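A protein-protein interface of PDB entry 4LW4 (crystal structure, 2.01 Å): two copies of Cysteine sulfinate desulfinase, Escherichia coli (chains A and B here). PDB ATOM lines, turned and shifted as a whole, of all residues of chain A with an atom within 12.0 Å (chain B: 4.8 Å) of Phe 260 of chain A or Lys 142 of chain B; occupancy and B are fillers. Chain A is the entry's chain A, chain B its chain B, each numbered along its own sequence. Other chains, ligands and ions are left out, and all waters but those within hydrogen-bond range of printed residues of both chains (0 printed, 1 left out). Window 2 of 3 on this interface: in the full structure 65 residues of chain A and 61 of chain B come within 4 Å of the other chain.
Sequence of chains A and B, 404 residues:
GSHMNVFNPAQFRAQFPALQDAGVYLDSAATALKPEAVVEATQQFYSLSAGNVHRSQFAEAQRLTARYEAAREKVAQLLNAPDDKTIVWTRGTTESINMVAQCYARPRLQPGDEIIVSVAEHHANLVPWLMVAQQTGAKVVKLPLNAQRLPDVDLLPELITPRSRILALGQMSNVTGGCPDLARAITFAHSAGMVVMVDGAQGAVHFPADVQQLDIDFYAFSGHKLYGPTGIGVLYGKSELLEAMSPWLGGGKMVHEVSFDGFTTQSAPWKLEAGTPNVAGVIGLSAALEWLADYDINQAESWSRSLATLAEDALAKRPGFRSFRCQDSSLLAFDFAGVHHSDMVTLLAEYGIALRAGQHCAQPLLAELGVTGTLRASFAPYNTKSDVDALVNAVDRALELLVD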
ATOM      1  N   VAL A 255       7.645   7.790 -14.793  1.00  0.00           N
ATOM      2  CA  VAL A 255       8.389   8.786 -15.539  1.00  0.00           C
ATOM      3  C   VAL A 255       7.415   9.950 -15.891  1.00  0.00           C
ATOM      4  O   VAL A 255       6.209   9.754 -16.026  1.00  0.00           O
ATOM      5  CB  VAL A 255       8.930   8.025 -16.780  1.00  0.00           C
ATOM      6  CG1 VAL A 255       8.068   8.263 -17.979  1.00  0.00           C
ATOM      7  CG2 VAL A 255      10.386   8.230 -17.007  1.00  0.00           C
ATOM      8  N   HIS A 256       7.905  11.169 -15.960  1.00  0.00           N
ATOM      9  CA  HIS A 256       7.089  12.257 -16.530  1.00  0.00           C
ATOM     10  C   HIS A 256       7.529  12.489 -18.009  1.00  0.00           C
ATOM     11  O   HIS A 256       6.798  12.152 -18.973  1.00  0.00           O
ATOM     12  CB  HIS A 256       7.304  13.499 -15.641  1.00  0.00           C
ATOM     13  CG  HIS A 256       6.758  14.767 -16.219  1.00  0.00           C
ATOM     14  ND1 HIS A 256       5.461  14.892 -16.642  1.00  0.00           N
ATOM     15  CD2 HIS A 256       7.317  15.996 -16.356  1.00  0.00           C
ATOM     16  CE1 HIS A 256       5.263  16.119 -17.101  1.00  0.00           C
ATOM     17  NE2 HIS A 256       6.369  16.810 -16.931  1.00  0.00           N
ATOM     18  N   GLU A 257       8.755  12.987 -18.181  1.00  0.00           N
ATOM     19  CA  GLU A 257       9.341  13.137 -19.531  1.00  0.00           C
ATOM     20  C   GLU A 257      10.559  12.292 -19.712  1.00  0.00           C
ATOM     21  O   GLU A 257      11.402  12.163 -18.769  1.00  0.00           O
ATOM     22  CB  GLU A 257       9.682  14.607 -19.824  1.00  0.00           C
ATOM     23  CG  GLU A 257       8.353  15.412 -19.765  1.00  0.00           C
ATOM     24  CD  GLU A 257       8.450  16.870 -20.268  1.00  0.00           C
ATOM     25  OE1 GLU A 257       9.436  17.556 -19.949  1.00  0.00           O
ATOM     26  OE2 GLU A 257       7.492  17.313 -20.947  1.00  0.00           O
ATOM     27  N   VAL A 258      10.690  11.782 -20.931  1.00  0.00           N
ATOM     28  CA  VAL A 258      11.797  10.928 -21.295  1.00  0.00           C
ATOM     29  C   VAL A 258      12.360  11.263 -22.675  1.00  0.00           C
ATOM     30  O   VAL A 258      11.592  11.379 -23.622  1.00  0.00           O
ATOM     31  CB  VAL A 258      11.368   9.400 -21.487  1.00  0.00           C
ATOM     32  CG1 VAL A 258      12.656   8.552 -21.423  1.00  0.00           C
ATOM     33  CG2 VAL A 258      10.394   8.956 -20.508  1.00  0.00           C
ATOM     34  N   SER A 259      13.674  11.324 -22.811  1.00  0.00           N
ATOM     35  CA  SER A 259      14.278  11.401 -24.147  1.00  0.00           C
ATOM     36  C   SER A 259      15.592  10.664 -24.073  1.00  0.00           C
ATOM     37  O   SER A 259      15.945  10.181 -22.976  1.00  0.00           O
ATOM     38  CB  SER A 259      14.511  12.884 -24.512  1.00  0.00           C
ATOM     39  OG  SER A 259      15.537  13.375 -23.679  1.00  0.00           O
ATOM     40  N   PHE A 260      16.343  10.573 -25.192  1.00  0.00           N
ATOM     41  CA  PHE A 260      17.678   9.998 -25.144  1.00  0.00           C
ATOM     42  C   PHE A 260      18.700  10.798 -24.332  1.00  0.00           C
ATOM     43  O   PHE A 260      19.792  10.296 -24.072  1.00  0.00           O
ATOM     44  CB  PHE A 260      18.213   9.625 -26.551  1.00  0.00           C
ATOM     45  CG  PHE A 260      17.629   8.303 -27.045  1.00  0.00           C
ATOM     46  CD1 PHE A 260      16.274   8.215 -27.398  1.00  0.00           C
ATOM     47  CD2 PHE A 260      18.397   7.149 -27.044  1.00  0.00           C
ATOM     48  CE1 PHE A 260      15.689   6.972 -27.789  1.00  0.00           C
ATOM     49  CE2 PHE A 260      17.833   5.895 -27.452  1.00  0.00           C
ATOM     50  CZ  PHE A 260      16.468   5.841 -27.841  1.00  0.00           C
ATOM     51  N   ASP A 261      18.303  11.974 -23.862  1.00  0.00           N
ATOM     52  CA  ASP A 261      19.152  12.741 -22.972  1.00  0.00           C
ATOM     53  C   ASP A 261      18.877  12.493 -21.498  1.00  0.00           C
ATOM     54  O   ASP A 261      19.701  12.860 -20.676  1.00  0.00           O
ATOM     55  CB  ASP A 261      19.069  14.267 -23.270  1.00  0.00           C
ATOM     56  CG  ASP A 261      19.439  14.585 -24.687  1.00  0.00           C
ATOM     57  OD1 ASP A 261      20.489  14.093 -25.142  1.00  0.00           O
ATOM     58  OD2 ASP A 261      18.675  15.293 -25.368  1.00  0.00           O
ATOM     59  N   GLY A 262      17.758  11.881 -21.131  1.00  0.00           N
ATOM     60  CA  GLY A 262      17.479  11.716 -19.681  1.00  0.00           C
ATOM     61  C   GLY A 262      15.992  11.733 -19.479  1.00  0.00           C
ATOM     62  O   GLY A 262      15.239  11.753 -20.469  1.00  0.00           O
ATOM     63  N   PHE A 263      15.576  11.743 -18.212  1.00  0.00           N
ATOM     64  CA  PHE A 263      14.174  11.634 -17.873  1.00  0.00           C
ATOM     65  C   PHE A 263      13.860  12.392 -16.586  1.00  0.00           C
ATOM     66  O   PHE A 263      14.706  12.618 -15.762  1.00  0.00           O
ATOM     67  CB  PHE A 263      13.734  10.149 -17.725  1.00  0.00           C
ATOM     68  CG  PHE A 263      14.419   9.435 -16.592  1.00  0.00           C
ATOM     69  CD1 PHE A 263      15.664   8.861 -16.775  1.00  0.00           C
ATOM     70  CD2 PHE A 263      13.819   9.380 -15.339  1.00  0.00           C
ATOM     71  CE1 PHE A 263      16.342   8.228 -15.711  1.00  0.00           C
ATOM     72  CE2 PHE A 263      14.475   8.739 -14.241  1.00  0.00           C
ATOM     73  CZ  PHE A 263      15.769   8.151 -14.450  1.00  0.00           C
ATOM     74  N   THR A 264      12.601  12.729 -16.409  1.00  0.00           N
ATOM     75  CA  THR A 264      12.152  13.297 -15.147  1.00  0.00           C
ATOM     76  C   THR A 264      11.071  12.356 -14.692  1.00  0.00           C
ATOM     77  O   THR A 264      10.567  11.587 -15.516  1.00  0.00           O
ATOM     78  CB  THR A 264      11.576  14.674 -15.368  1.00  0.00           C
ATOM     79  OG1 THR A 264      10.570  14.593 -16.388  1.00  0.00           O
ATOM     80  CG2 THR A 264      12.720  15.635 -15.817  1.00  0.00           C
ATOM     81  N   VAL B 117      20.062   1.678 -27.817  1.00  0.00           N
ATOM     82  CA  VAL B 117      18.629   1.533 -27.496  1.00  0.00           C
ATOM     83  C   VAL B 117      17.869   2.081 -28.719  1.00  0.00           C
ATOM     84  O   VAL B 117      18.104   3.231 -29.158  1.00  0.00           O
ATOM     85  CB  VAL B 117      18.220   2.339 -26.219  1.00  0.00           C
ATOM     86  CG1 VAL B 117      16.768   2.177 -25.904  1.00  0.00           C
ATOM     87  CG2 VAL B 117      19.032   1.828 -24.943  1.00  0.00           C
ATOM     88  N   SER B 118      16.984   1.263 -29.275  1.00  0.00           N
ATOM     89  CA  SER B 118      16.184   1.763 -30.397  1.00  0.00           C
ATOM     90  C   SER B 118      15.279   2.934 -30.046  1.00  0.00           C
ATOM     91  O   SER B 118      14.741   3.058 -28.961  1.00  0.00           O
ATOM     92  CB  SER B 118      15.478   0.614 -31.176  1.00  0.00           C
ATOM     93  OG  SER B 118      14.124   0.651 -30.916  1.00  0.00           O
ATOM     94  N   VAL B 119      15.076   3.818 -31.007  1.00  0.00           N
ATOM     95  CA  VAL B 119      14.178   4.923 -30.760  1.00  0.00           C
ATOM     96  C   VAL B 119      12.709   4.449 -30.655  1.00  0.00           C
ATOM     97  O   VAL B 119      11.891   5.160 -30.115  1.00  0.00           O
ATOM     98  CB  VAL B 119      14.400   6.088 -31.813  1.00  0.00           C
ATOM     99  CG1 VAL B 119      14.003   5.602 -33.207  1.00  0.00           C
ATOM    100  CG2 VAL B 119      13.635   7.336 -31.402  1.00  0.00           C
ATOM    101  N   LEU B 126      14.003   1.606 -22.051  1.00  0.00           N
ATOM    102  CA  LEU B 126      14.845   2.795 -22.267  1.00  0.00           C
ATOM    103  C   LEU B 126      15.281   3.390 -20.918  1.00  0.00           C
ATOM    104  O   LEU B 126      16.443   3.552 -20.661  1.00  0.00           O
ATOM    105  CB  LEU B 126      14.101   3.857 -23.137  1.00  0.00           C
ATOM    106  CG  LEU B 126      14.828   5.231 -23.137  1.00  0.00           C
ATOM    107  CD1 LEU B 126      16.334   5.164 -23.676  1.00  0.00           C
ATOM    108  CD2 LEU B 126      13.999   6.273 -23.923  1.00  0.00           C
ATOM    109  N   LEU B 130      18.902   4.365 -19.275  1.00  0.00           N
ATOM    110  CA  LEU B 130      19.383   5.714 -18.898  1.00  0.00           C
ATOM    111  C   LEU B 130      19.906   5.720 -17.443  1.00  0.00           C
ATOM    112  O   LEU B 130      20.915   6.340 -17.155  1.00  0.00           O
ATOM    113  CB  LEU B 130      18.274   6.791 -19.061  1.00  0.00           C
ATOM    114  CG  LEU B 130      17.846   7.025 -20.537  1.00  0.00           C
ATOM    115  CD1 LEU B 130      16.493   7.747 -20.580  1.00  0.00           C
ATOM    116  CD2 LEU B 130      18.832   7.799 -21.380  1.00  0.00           C
ATOM    117  N   VAL B 140      23.856   5.931 -23.318  1.00  0.00           N
ATOM    118  CA  VAL B 140      22.818   5.449 -24.206  1.00  0.00           C
ATOM    119  C   VAL B 140      22.987   6.087 -25.602  1.00  0.00           C
ATOM    120  O   VAL B 140      23.042   7.290 -25.698  1.00  0.00           O
ATOM    121  CB  VAL B 140      21.404   5.745 -23.626  1.00  0.00           C
ATOM    122  CG1 VAL B 140      20.283   5.272 -24.637  1.00  0.00           C
ATOM    123  CG2 VAL B 140      21.284   4.994 -22.308  1.00  0.00           C
ATOM    124  N   VAL B 141      23.085   5.244 -26.627  1.00  0.00           N
ATOM    125  CA  VAL B 141      23.177   5.623 -28.041  1.00  0.00           C
ATOM    126  C   VAL B 141      21.880   5.217 -28.776  1.00  0.00           C
ATOM    127  O   VAL B 141      21.431   4.073 -28.697  1.00  0.00           O
ATOM    128  CB  VAL B 141      24.459   5.021 -28.705  1.00  0.00           C
ATOM    129  CG1 VAL B 141      24.604   5.482 -30.147  1.00  0.00           C
ATOM    130  CG2 VAL B 141      25.698   5.515 -27.947  1.00  0.00           C
ATOM    131  N   LYS B 142      21.320   6.156 -29.526  1.00  0.00           N
ATOM    132  CA  LYS B 142      20.075   5.971 -30.253  1.00  0.00           C
ATOM    133  C   LYS B 142      20.249   5.088 -31.513  1.00  0.00           C
ATOM    134  O   LYS B 142      21.181   5.249 -32.333  1.00  0.00           O
ATOM    135  CB  LYS B 142      19.432   7.361 -30.583  1.00  0.00           C
ATOM    136  CG  LYS B 142      18.080   7.286 -31.343  1.00  0.00           C
ATOM    137  CD  LYS B 142      17.574   8.650 -31.899  1.00  0.00           C
ATOM    138  CE  LYS B 142      17.381   9.680 -30.805  1.00  0.00           C
ATOM    139  NZ  LYS B 142      16.905  11.014 -31.323  1.00  0.00           N
ATOM    140  N   LEU B 143      19.402   4.093 -31.659  1.00  0.00           N
ATOM    141  CA  LEU B 143      19.344   3.360 -32.960  1.00  0.00           C
ATOM    142  C   LEU B 143      18.076   3.958 -33.653  1.00  0.00           C
ATOM    143  O   LEU B 143      16.957   3.795 -33.161  1.00  0.00           O
ATOM    144  CB  LEU B 143      19.305   1.819 -32.726  1.00  0.00           C
ATOM    145  CG  LEU B 143      18.927   0.938 -33.930  1.00  0.00           C
ATOM    146  CD1 LEU B 143      20.120   0.979 -34.912  1.00  0.00           C
ATOM    147  CD2 LEU B 143      18.669  -0.505 -33.577  1.00  0.00           C
ATOM    148  N   PRO B 144      18.270   4.798 -34.717  1.00  0.00           N
ATOM    149  CA  PRO B 144      17.125   5.424 -35.404  1.00  0.00           C
ATOM    150  C   PRO B 144      16.300   4.433 -36.235  1.00  0.00           C
ATOM    151  O   PRO B 144      16.713   3.306 -36.467  1.00  0.00           O
ATOM    152  CB  PRO B 144      17.769   6.442 -36.434  1.00  0.00           C
ATOM    153  CG  PRO B 144      19.140   6.449 -36.249  1.00  0.00           C
ATOM    154  CD  PRO B 144      19.565   5.267 -35.264  1.00  0.00           C
ATOM    155  N   LEU B 159      27.186   2.067 -35.783  1.00  0.00           N
ATOM    156  CA  LEU B 159      26.938   2.558 -34.451  1.00  0.00           C
ATOM    157  C   LEU B 159      27.721   1.769 -33.440  1.00  0.00           C
ATOM    158  O   LEU B 159      27.915   2.207 -32.321  1.00  0.00           O
ATOM    159  CB  LEU B 159      25.425   2.491 -34.149  1.00  0.00           C
ATOM    160  CG  LEU B 159      24.675   3.667 -34.775  1.00  0.00           C
ATOM    161  CD1 LEU B 159      23.225   3.330 -34.840  1.00  0.00           C
ATOM    162  CD2 LEU B 159      24.878   4.980 -33.986  1.00  0.00           C
ATOM    163  N   PRO B 364       9.964   9.020 -27.227  1.00  0.00           N
ATOM    164  CA  PRO B 364      10.914   9.201 -28.316  1.00  0.00           C
ATOM    165  C   PRO B 364      10.396   8.762 -29.649  1.00  0.00           C
ATOM    166  O   PRO B 364      10.674   9.429 -30.643  1.00  0.00           O
ATOM    167  CB  PRO B 364      12.157   8.372 -27.893  1.00  0.00           C
ATOM    168  CG  PRO B 364      12.072   8.454 -26.386  1.00  0.00           C
ATOM    169  CD  PRO B 364      10.596   8.319 -26.092  1.00  0.00           C
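Among the printed residues, merely in contact across the chains: Phe 260 of chain A with Val 117 of chain B (3.2 Å), Ser 259 of chain A with Leu 130 of chain B (3.5 Å), Phe 260 of chain A with Ser 118 of chain B (3.5 Å), Phe 260 of chain A with Val 140 of chain B (3.6 Å), Phe 260 of chain A with Lys 142 of chain B (3.6 Å), Val 258 of chain A with Leu 126 of chain B (3.6 Å), Phe 260 of chain A with Leu 130 of chain B (3.8 Å), Phe 260 of chain A with Pro 364 of chain B (3.8 Å) and Phe 260 of chain A with Val 119 of chain B (3.8 Å).
Of the 12 printed residues of chain B, 8 touch a printed residue of chain A.
Printed residues of chain B that touch a printed residue of chain A: Val 117, Ser 118, Val 119, Leu 126, Leu 130, Val 140, Lys 142 and Pro 364.
Printed residues of chain A that touch a printed residue of chain B: Val 258, Ser 259 and Phe 260.
Hydrophobic or aromatic side chains of chain A that line the printed part of chain B: Val 258 and Phe 260.
Among the printed residues, 9 pairs touch across the chains.
Among the printed residues, no Asp or Glu carboxylate lies within 4 Å of a Lys or Arg side-chain nitrogen of the other chain.
O of Val 141 of chain B sits at hydrogen-bond distance from N of Val 117 of chain B (2.9 Å).
OG of Ser 259 of chain A lies close to N of Asp 261 of chain A.
The backbone NH (N) of Val 119 of chain B is in hydrogen-bond range of the backbone carbonyl oxygen (O) of Leu 143 of chain B, at 2.9 Å.
O of Val 117 of chain B is in hydrogen-bond range of N of Leu 143 of chain B (2.9 Å).
Printed residues of chain B within 4 Å of Val 258 of chain A: Leu 126 (3.6 Å).
Of the printed residues of chain B, Ser 259 of chain A touches Leu 130 (3.5 Å).
Phe 260 of chain A touches just these residues of chain B: Val 117 (3.2 Å), Ser 118 (3.5 Å), Val 119 (3.8 Å), Leu 130 (3.8 Å), Val 140 (3.6 Å), Lys 142 (3.6 Å) and Pro 364 (3.8 Å).
Ser 118 of chain B touches just one residue of chain A: Phe 260 (3.5 Å).
Of the printed residues of chain A, Leu 130 of chain B touches Ser 259 and Phe 260.
Of chain A, only Phe 260 (3.6 Å) comes within 4 Å of Val 140 of chain B.
No residue of chain A comes within 4 Å of Val 141 of chain B.
Lys 142 of chain B touches one residue of chain A.
No residue of chain A comes within 4 Å of Leu 143 of chain B.
The nearest residue of chain A that does not touch Lys 142 of chain B is Ser 259 of chain A (7.0 Å).
No position is printed for both chains.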
